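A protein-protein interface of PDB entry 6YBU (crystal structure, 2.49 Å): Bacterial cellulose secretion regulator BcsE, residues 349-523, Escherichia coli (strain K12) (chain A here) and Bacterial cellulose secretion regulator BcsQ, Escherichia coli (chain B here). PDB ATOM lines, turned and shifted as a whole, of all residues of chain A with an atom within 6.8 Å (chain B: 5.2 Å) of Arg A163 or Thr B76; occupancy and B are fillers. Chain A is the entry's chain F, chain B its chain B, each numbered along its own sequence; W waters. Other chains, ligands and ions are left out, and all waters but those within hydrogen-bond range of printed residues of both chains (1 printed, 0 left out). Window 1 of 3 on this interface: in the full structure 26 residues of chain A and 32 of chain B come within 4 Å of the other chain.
O of Tyr B75 lies within hydrogen-bond range of ND2 of Asn A153 (3.0 Å). NH1 of Arg A163 is in salt-bridge range of OE2 of Glu B217 (3.4 Å). OE1 of Gln B78 sits at hydrogen-bond distance from NZ of Lys A149 (3.5 Å). ND2 of Asn B49 sits at hydrogen-bond distance from O of Arg A163 (2.8 Å). The side-chain amide nitrogen of Gln A146 is in hydrogen-bond range of the side-chain amide oxygen of Gln B78 (3.1 Å).
The side-chain hydroxyl (OH) of Tyr B75 lies within hydrogen-bond range of the side-chain carboxylate (OE1) of Glu B217. O of Gln B27 lies close to OE1 of Gln B78 (3.5 Å). The side-chain hydroxyl (OG1) of Thr B76 is in hydrogen-bond range of the side-chain amide oxygen (OE1) of Gln B27 (3.0 Å). O of Trp B24 sits at hydrogen-bond distance from NE2 of Gln B27, 3.0 Å away. The backbone carbonyl oxygen (O) of Asn A153 lies within hydrogen-bond range of the backbone NH (N) of Ile A164 (2.8 Å). OE1 of Gln A146 sits at hydrogen-bond distance from NZ of Lys A149 (3.3 Å).
NE2 of Gln A146 touches O of Gln B27, 3.6 Å away. NH2 of Arg A162 touches OD1 of Asn B49 (3.5 Å). NH1 of Arg A163 touches CH2 of Trp B24, 3.4 Å away. Arg A163 touches Tyr B75 (CD to O, 3.6 Å). Thr B76 touches Arg A163. CD1 of Ile A164 touches ND2 of Asn B49, at 3.6 Å. Pro A165 touches Phe B48. CD of Pro A165 touches O of Asn B49 (3.7 Å). Arg B74 touches Pro A165.
Pro A150 touches none of the printed residues of chain B. Val A151 touches none of the printed residues of chain B. Printed residues of chain B within 4 Å of Arg A162: Asn B49. Arg A163 touches five residues of chain B. Printed residues of chain A within 4 Å of Phe B48: Pro A165. Of chain A, only Arg A163 comes within 4 Å of Thr B76. Printed residues of chain A within 4 Å of Gln B78: Gln A146 (3.1 Å) and Lys A149 (3.5 Å). The nearest residue of chain B that does not touch Arg A163 is Phe B48 (4.8 Å). The nearest residue of chain A that does not touch Thr B76 is Asn A153 (5.1 Å). The nearest printed residue of chain A that does not touch Phe B48 is Arg A163 (4.8 Å).
Of the 12 printed residues of chain B, 9 touch a printed residue of chain A. Of the 13 printed residues of chain A, 7 touch a printed residue of chain B. Hydrophobic or aromatic side chains of chain A within 4 Å of the printed part of chain B: Ile A164 and Pro A165. Among the printed residues, Asp or Glu carboxylates within 4 Å of a Lys or Arg side-chain nitrogen of the other chain: Arg A163 with Glu B217.
Water W1 lies within hydrogen-bond range of N of Arg A163, OE2 of Glu B217 and OH of Tyr B75.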
ATOM      1  N   GLN A 146      16.077  19.962 -13.546  1.00  0.00           N
ATOM      2  CA  GLN A 146      16.229  18.838 -14.464  1.00  0.00           C
ATOM      3  C   GLN A 146      17.443  19.017 -15.367  1.00  0.00           C
ATOM      4  O   GLN A 146      18.015  18.029 -15.841  1.00  0.00           O
ATOM      5  CB  GLN A 146      14.963  18.661 -15.305  1.00  0.00           C
ATOM      6  CG  GLN A 146      13.747  18.169 -14.530  1.00  0.00           C
ATOM      7  CD  GLN A 146      13.794  16.680 -14.226  1.00  0.00           C
ATOM      8  OE1 GLN A 146      14.790  16.006 -14.497  1.00  0.00           O
ATOM      9  NE2 GLN A 146      12.709  16.157 -13.666  1.00  0.00           N
ATOM     10  N   SER A 147      17.848  20.263 -15.617  1.00  0.00           N
ATOM     11  CA  SER A 147      19.048  20.511 -16.405  1.00  0.00           C
ATOM     12  C   SER A 147      20.313  20.409 -15.564  1.00  0.00           C
ATOM     13  O   SER A 147      21.390  20.131 -16.104  1.00  0.00           O
ATOM     14  CB  SER A 147      18.970  21.886 -17.066  1.00  0.00           C
ATOM     15  OG  SER A 147      17.873  21.962 -17.960  1.00  0.00           O
ATOM     16  N   LYS A 149      20.795  18.082 -13.519  1.00  0.00           N
ATOM     17  CA  LYS A 149      21.059  16.665 -13.348  1.00  0.00           C
ATOM     18  C   LYS A 149      22.152  16.213 -14.314  1.00  0.00           C
ATOM     19  O   LYS A 149      22.346  16.819 -15.372  1.00  0.00           O
ATOM     20  CB  LYS A 149      19.791  15.848 -13.588  1.00  0.00           C
ATOM     21  CG  LYS A 149      18.769  15.909 -12.467  1.00  0.00           C
ATOM     22  CD  LYS A 149      17.585  15.004 -12.774  1.00  0.00           C
ATOM     23  CE  LYS A 149      16.587  14.974 -11.628  1.00  0.00           C
ATOM     24  NZ  LYS A 149      15.444  14.062 -11.920  1.00  0.00           N
ATOM     25  N   PRO A 150      22.886  15.160 -13.971  1.00  0.00           N
ATOM     26  CA  PRO A 150      23.885  14.623 -14.900  1.00  0.00           C
ATOM     27  C   PRO A 150      23.224  14.059 -16.149  1.00  0.00           C
ATOM     28  O   PRO A 150      22.016  13.818 -16.208  1.00  0.00           O
ATOM     29  CB  PRO A 150      24.578  13.522 -14.091  1.00  0.00           C
ATOM     30  CG  PRO A 150      24.311  13.873 -12.668  1.00  0.00           C
ATOM     31  CD  PRO A 150      22.949  14.496 -12.658  1.00  0.00           C
ATOM     32  N   VAL A 151      24.051  13.846 -17.166  1.00  0.00           N
ATOM     33  CA  VAL A 151      23.614  13.268 -18.430  1.00  0.00           C
ATOM     34  C   VAL A 151      24.584  12.150 -18.795  1.00  0.00           C
ATOM     35  O   VAL A 151      25.706  12.415 -19.243  1.00  0.00           O
ATOM     36  CB  VAL A 151      23.533  14.317 -19.547  1.00  0.00           C
ATOM     37  CG1 VAL A 151      22.233  15.093 -19.444  1.00  0.00           C
ATOM     38  CG2 VAL A 151      24.713  15.286 -19.462  1.00  0.00           C
ATOM     39  N   ASN A 153      24.468  10.046 -21.209  1.00  0.00           N
ATOM     40  CA  ASN A 153      24.407   9.646 -22.612  1.00  0.00           C
ATOM     41  C   ASN A 153      24.465  10.845 -23.551  1.00  0.00           C
ATOM     42  O   ASN A 153      23.951  10.786 -24.676  1.00  0.00           O
ATOM     43  CB  ASN A 153      23.143   8.831 -22.905  1.00  0.00           C
ATOM     44  CG  ASN A 153      21.876   9.550 -22.485  1.00  0.00           C
ATOM     45  OD1 ASN A 153      21.839  10.188 -21.433  1.00  0.00           O
ATOM     46  ND2 ASN A 153      20.830   9.455 -23.304  1.00  0.00           N
ATOM     47  N   ALA A 154      25.088  11.931 -23.114  1.00  0.00           N
ATOM     48  CA  ALA A 154      25.193  13.115 -23.939  1.00  0.00           C
ATOM     49  C   ALA A 154      26.326  12.958 -24.943  1.00  0.00           C
ATOM     50  O   ALA A 154      27.260  12.174 -24.757  1.00  0.00           O
ATOM     51  CB  ALA A 154      25.419  14.351 -23.072  1.00  0.00           C
ATOM     52  N   GLU A 155      26.225  13.725 -26.023  1.00  0.00           N
ATOM     53  CA  GLU A 155      27.218  13.707 -27.085  1.00  0.00           C
ATOM     54  C   GLU A 155      27.076  15.004 -27.865  1.00  0.00           C
ATOM     55  O   GLU A 155      25.974  15.343 -28.310  1.00  0.00           O
ATOM     56  CB  GLU A 155      27.025  12.488 -27.993  1.00  0.00           C
ATOM     57  CG  GLU A 155      28.193  12.197 -28.918  1.00  0.00           C
ATOM     58  CD  GLU A 155      27.966  10.957 -29.771  1.00  0.00           C
ATOM     59  OE1 GLU A 155      28.292   9.840 -29.311  1.00  0.00           O
ATOM     60  OE2 GLU A 155      27.450  11.100 -30.900  1.00  0.00           O
ATOM     61  N   TRP A 161      24.378  19.906 -27.645  1.00  0.00           N
ATOM     62  CA  TRP A 161      24.372  18.617 -26.970  1.00  0.00           C
ATOM     63  C   TRP A 161      23.221  17.765 -27.490  1.00  0.00           C
ATOM     64  O   TRP A 161      22.084  18.236 -27.594  1.00  0.00           O
ATOM     65  CB  TRP A 161      24.232  18.792 -25.457  1.00  0.00           C
ATOM     66  CG  TRP A 161      25.445  19.337 -24.763  1.00  0.00           C
ATOM     67  CD1 TRP A 161      25.588  20.580 -24.218  1.00  0.00           C
ATOM     68  CD2 TRP A 161      26.682  18.651 -24.526  1.00  0.00           C
ATOM     69  NE1 TRP A 161      26.836  20.714 -23.660  1.00  0.00           N
ATOM     70  CE2 TRP A 161      27.528  19.545 -23.835  1.00  0.00           C
ATOM     71  CE3 TRP A 161      27.158  17.371 -24.832  1.00  0.00           C
ATOM     72  CZ2 TRP A 161      28.820  19.202 -23.448  1.00  0.00           C
ATOM     73  CZ3 TRP A 161      28.443  17.033 -24.444  1.00  0.00           C
ATOM     74  CH2 TRP A 161      29.259  17.946 -23.759  1.00  0.00           C
ATOM     75  N   ARG A 162      23.515  16.509 -27.804  1.00  0.00           N
ATOM     76  CA  ARG A 162      22.510  15.548 -28.227  1.00  0.00           C
ATOM     77  C   ARG A 162      22.540  14.337 -27.307  1.00  0.00           C
ATOM     78  O   ARG A 162      23.598  13.934 -26.816  1.00  0.00           O
ATOM     79  CB  ARG A 162      22.733  15.101 -29.677  1.00  0.00           C
ATOM     80  CG  ARG A 162      22.767  16.243 -30.675  1.00  0.00           C
ATOM     81  CD  ARG A 162      22.732  15.737 -32.108  1.00  0.00           C
ATOM     82  NE  ARG A 162      21.499  15.017 -32.409  1.00  0.00           N
ATOM     83  CZ  ARG A 162      20.352  15.605 -32.731  1.00  0.00           C
ATOM     84  NH1 ARG A 162      20.274  16.928 -32.787  1.00  0.00           N
ATOM     85  NH2 ARG A 162      19.281  14.869 -32.991  1.00  0.00           N
ATOM     86  N   ARG A 163      21.366  13.764 -27.075  1.00  0.00           N
ATOM     87  CA  ARG A 163      21.237  12.561 -26.270  1.00  0.00           C
ATOM     88  C   ARG A 163      21.326  11.328 -27.157  1.00  0.00           C
ATOM     89  O   ARG A 163      20.821  11.319 -28.283  1.00  0.00           O
ATOM     90  CB  ARG A 163      19.915  12.565 -25.504  1.00  0.00           C
ATOM     91  CG  ARG A 163      19.900  13.521 -24.328  1.00  0.00           C
ATOM     92  CD  ARG A 163      18.584  13.460 -23.577  1.00  0.00           C
ATOM     93  NE  ARG A 163      18.730  13.891 -22.190  1.00  0.00           N
ATOM     94  CZ  ARG A 163      18.636  15.153 -21.783  1.00  0.00           C
ATOM     95  NH1 ARG A 163      18.395  16.120 -22.659  1.00  0.00           N
ATOM     96  NH2 ARG A 163      18.785  15.444 -20.497  1.00  0.00           N
ATOM     97  N   ILE A 164      21.973  10.289 -26.643  1.00  0.00           N
ATOM     98  CA  ILE A 164      22.137   9.021 -27.341  1.00  0.00           C
ATOM     99  C   ILE A 164      21.299   7.978 -26.606  1.00  0.00           C
ATOM    100  O   ILE A 164      21.591   7.662 -25.443  1.00  0.00           O
ATOM    101  CB  ILE A 164      23.611   8.603 -27.416  1.00  0.00           C
ATOM    102  CG1 ILE A 164      24.443   9.701 -28.083  1.00  0.00           C
ATOM    103  CG2 ILE A 164      23.752   7.292 -28.164  1.00  0.00           C
ATOM    104  CD1 ILE A 164      23.979  10.054 -29.481  1.00  0.00           C
ATOM    105  N   PRO A 165      20.248   7.440 -27.219  1.00  0.00           N
ATOM    106  CA  PRO A 165      19.456   6.402 -26.545  1.00  0.00           C
ATOM    107  C   PRO A 165      20.295   5.161 -26.278  1.00  0.00           C
ATOM    108  O   PRO A 165      21.022   4.679 -27.151  1.00  0.00           O
ATOM    109  CB  PRO A 165      18.319   6.124 -27.535  1.00  0.00           C
ATOM    110  CG  PRO A 165      18.833   6.603 -28.857  1.00  0.00           C
ATOM    111  CD  PRO A 165      19.716   7.772 -28.550  1.00  0.00           C
ATOM    112  N   TRP B  24       8.266  14.027 -23.627  1.00  0.00           N
ATOM    113  CA  TRP B  24       9.345  14.880 -23.139  1.00  0.00           C
ATOM    114  C   TRP B  24       8.852  15.828 -22.054  1.00  0.00           C
ATOM    115  O   TRP B  24       9.574  16.104 -21.090  1.00  0.00           O
ATOM    116  CB  TRP B  24       9.962  15.670 -24.290  1.00  0.00           C
ATOM    117  CG  TRP B  24      10.968  16.672 -23.816  1.00  0.00           C
ATOM    118  CD1 TRP B  24      10.758  18.003 -23.581  1.00  0.00           C
ATOM    119  CD2 TRP B  24      12.339  16.421 -23.497  1.00  0.00           C
ATOM    120  NE1 TRP B  24      11.919  18.594 -23.144  1.00  0.00           N
ATOM    121  CE2 TRP B  24      12.904  17.644 -23.083  1.00  0.00           C
ATOM    122  CE3 TRP B  24      13.148  15.280 -23.524  1.00  0.00           C
ATOM    123  CZ2 TRP B  24      14.237  17.757 -22.701  1.00  0.00           C
ATOM    124  CZ3 TRP B  24      14.470  15.396 -23.143  1.00  0.00           C
ATOM    125  CH2 TRP B  24      15.002  16.624 -22.739  1.00  0.00           C
ATOM    126  N   GLN B  27       8.278  13.754 -18.674  1.00  0.00           N
ATOM    127  CA  GLN B  27       9.527  13.445 -17.984  1.00  0.00           C
ATOM    128  C   GLN B  27      10.194  14.708 -17.455  1.00  0.00           C
ATOM    129  O   GLN B  27      10.890  14.657 -16.435  1.00  0.00           O
ATOM    130  CB  GLN B  27      10.475  12.670 -18.908  1.00  0.00           C
ATOM    131  CG  GLN B  27      11.039  13.461 -20.087  1.00  0.00           C
ATOM    132  CD  GLN B  27      12.280  14.265 -19.726  1.00  0.00           C
ATOM    133  OE1 GLN B  27      13.111  13.825 -18.933  1.00  0.00           O
ATOM    134  NE2 GLN B  27      12.400  15.456 -20.301  1.00  0.00           N
ATOM    135  N   PHE B  48      13.729  10.733 -31.249  1.00  0.00           N
ATOM    136  CA  PHE B  48      14.584  10.541 -30.084  1.00  0.00           C
ATOM    137  C   PHE B  48      15.995  10.143 -30.496  1.00  0.00           C
ATOM    138  O   PHE B  48      16.671   9.399 -29.779  1.00  0.00           O
ATOM    139  CB  PHE B  48      13.989   9.504 -29.134  1.00  0.00           C
ATOM    140  CG  PHE B  48      12.687   9.923 -28.519  1.00  0.00           C
ATOM    141  CD1 PHE B  48      12.667  10.718 -27.384  1.00  0.00           C
ATOM    142  CD2 PHE B  48      11.482   9.525 -29.078  1.00  0.00           C
ATOM    143  CE1 PHE B  48      11.469  11.109 -26.816  1.00  0.00           C
ATOM    144  CE2 PHE B  48      10.280   9.910 -28.513  1.00  0.00           C
ATOM    145  CZ  PHE B  48      10.272  10.703 -27.380  1.00  0.00           C
ATOM    146  N   ASN B  49      16.442  10.622 -31.658  1.00  0.00           N
ATOM    147  CA  ASN B  49      17.820  10.456 -32.124  1.00  0.00           C
ATOM    148  C   ASN B  49      18.205   8.985 -32.272  1.00  0.00           C
ATOM    149  O   ASN B  49      19.375   8.621 -32.130  1.00  0.00           O
ATOM    150  CB  ASN B  49      18.803  11.182 -31.200  1.00  0.00           C
ATOM    151  CG  ASN B  49      20.132  11.471 -31.870  1.00  0.00           C
ATOM    152  OD1 ASN B  49      20.231  11.492 -33.097  1.00  0.00           O
ATOM    153  ND2 ASN B  49      21.165  11.695 -31.064  1.00  0.00           N
ATOM    154  N   ARG B  74      16.671   3.758 -23.395  1.00  0.00           N
ATOM    155  CA  ARG B  74      16.613   4.802 -22.381  1.00  0.00           C
ATOM    156  C   ARG B  74      17.044   6.124 -23.004  1.00  0.00           C
ATOM    157  O   ARG B  74      18.161   6.236 -23.520  1.00  0.00           O
ATOM    158  CB  ARG B  74      17.508   4.451 -21.194  1.00  0.00           C
ATOM    159  CG  ARG B  74      17.454   5.459 -20.058  1.00  0.00           C
ATOM    160  CD  ARG B  74      18.324   5.020 -18.888  1.00  0.00           C
ATOM    161  NE  ARG B  74      18.064   3.635 -18.508  1.00  0.00           N
ATOM    162  CZ  ARG B  74      17.055   3.246 -17.737  1.00  0.00           C
ATOM    163  NH1 ARG B  74      16.199   4.142 -17.260  1.00  0.00           N
ATOM    164  NH2 ARG B  74      16.897   1.960 -17.447  1.00  0.00           N
ATOM    165  N   TYR B  75      16.158   7.119 -22.964  1.00  0.00           N
ATOM    166  CA  TYR B  75      16.470   8.442 -23.491  1.00  0.00           C
ATOM    167  C   TYR B  75      16.926   9.402 -22.402  1.00  0.00           C
ATOM    168  O   TYR B  75      17.943  10.084 -22.563  1.00  0.00           O
ATOM    169  CB  TYR B  75      15.258   9.019 -24.230  1.00  0.00           C
ATOM    170  CG  TYR B  75      15.609  10.185 -25.122  1.00  0.00           C
ATOM    171  CD1 TYR B  75      16.398  10.004 -26.251  1.00  0.00           C
ATOM    172  CD2 TYR B  75      15.156  11.467 -24.836  1.00  0.00           C
ATOM    173  CE1 TYR B  75      16.728  11.063 -27.072  1.00  0.00           C
ATOM    174  CE2 TYR B  75      15.480  12.534 -25.650  1.00  0.00           C
ATOM    175  CZ  TYR B  75      16.266  12.326 -26.766  1.00  0.00           C
ATOM    176  OH  TYR B  75      16.591  13.386 -27.579  1.00  0.00           O
ATOM    177  N   THR B  76      16.185   9.481 -21.300  1.00  0.00           N
ATOM    178  CA  THR B  76      16.615  10.182 -20.096  1.00  0.00           C
ATOM    179  C   THR B  76      16.390   9.263 -18.902  1.00  0.00           C
ATOM    180  O   THR B  76      15.892   8.141 -19.040  1.00  0.00           O
ATOM    181  CB  THR B  76      15.873  11.512 -19.905  1.00  0.00           C
ATOM    182  OG1 THR B  76      14.484  11.262 -19.653  1.00  0.00           O
ATOM    183  CG2 THR B  76      16.010  12.395 -21.134  1.00  0.00           C
ATOM    184  N   SER B  77      16.757   9.751 -17.713  1.00  0.00           N
ATOM    185  CA  SER B  77      16.562   8.971 -16.496  1.00  0.00           C
ATOM    186  C   SER B  77      15.093   8.674 -16.224  1.00  0.00           C
ATOM    187  O   SER B  77      14.788   7.734 -15.481  1.00  0.00           O
ATOM    188  CB  SER B  77      17.180   9.704 -15.300  1.00  0.00           C
ATOM    189  OG  SER B  77      16.645  11.010 -15.171  1.00  0.00           O
ATOM    190  N   GLN B  78      14.175   9.445 -16.812  1.00  0.00           N
ATOM    191  CA  GLN B  78      12.747   9.269 -16.579  1.00  0.00           C
ATOM    192  C   GLN B  78      11.955   9.057 -17.865  1.00  0.00           C
ATOM    193  O   GLN B  78      10.719   9.118 -17.832  1.00  0.00           O
ATOM    194  CB  GLN B  78      12.182  10.471 -15.816  1.00  0.00           C
ATOM    195  CG  GLN B  78      12.887  10.754 -14.498  1.00  0.00           C
ATOM    196  CD  GLN B  78      12.328  11.974 -13.790  1.00  0.00           C
ATOM    197  OE1 GLN B  78      12.814  13.091 -13.974  1.00  0.00           O
ATOM    198  NE2 GLN B  78      11.300  11.765 -12.975  1.00  0.00           N
ATOM    199  N   LEU B  79      12.620   8.811 -18.993  1.00  0.00           N
ATOM    200  CA  LEU B  79      11.932   8.578 -20.258  1.00  0.00           C
ATOM    201  C   LEU B  79      12.574   7.396 -20.967  1.00  0.00           C
ATOM    202  O   LEU B  79      13.750   7.458 -21.337  1.00  0.00           O
ATOM    203  CB  LEU B  79      11.967   9.823 -21.151  1.00  0.00           C
ATOM    204  CG  LEU B  79      11.369   9.697 -22.557  1.00  0.00           C
ATOM    205  CD1 LEU B  79       9.975   9.088 -22.506  1.00  0.00           C
ATOM    206  CD2 LEU B  79      11.327  11.057 -23.241  1.00  0.00           C
ATOM    207  N   ASP B  80      11.799   6.329 -21.153  1.00  0.00           N
ATOM    208  CA  ASP B  80      12.220   5.151 -21.899  1.00  0.00           C
ATOM    209  C   ASP B  80      11.383   5.020 -23.165  1.00  0.00           C
ATOM    210  O   ASP B  80      10.209   5.399 -23.198  1.00  0.00           O
ATOM    211  CB  ASP B  80      12.090   3.878 -21.056  1.00  0.00           C
ATOM    212  CG  ASP B  80      13.068   3.841 -19.901  1.00  0.00           C
ATOM    213  OD1 ASP B  80      14.095   4.552 -19.964  1.00  0.00           O
ATOM    214  OD2 ASP B  80      12.811   3.097 -18.930  1.00  0.00           O
ATOM    215  N   GLU B 217      12.676  19.591 -26.274  1.00  0.00           N
ATOM    216  CA  GLU B 217      14.132  19.605 -26.204  1.00  0.00           C
ATOM    217  C   GLU B 217      14.732  20.490 -27.291  1.00  0.00           C
ATOM    218  O   GLU B 217      15.707  21.207 -27.043  1.00  0.00           O
ATOM    219  CB  GLU B 217      14.671  18.178 -26.321  1.00  0.00           C
ATOM    220  CG  GLU B 217      16.186  18.080 -26.272  1.00  0.00           C
ATOM    221  CD  GLU B 217      16.688  16.650 -26.388  1.00  0.00           C
ATOM    222  OE1 GLU B 217      15.901  15.773 -26.810  1.00  0.00           O
ATOM    223  OE2 GLU B 217      17.867  16.403 -26.052  1.00  0.00           O
HETATM  224  O   HOH W   1      19.122  14.810 -27.874  1.00  0.00           O
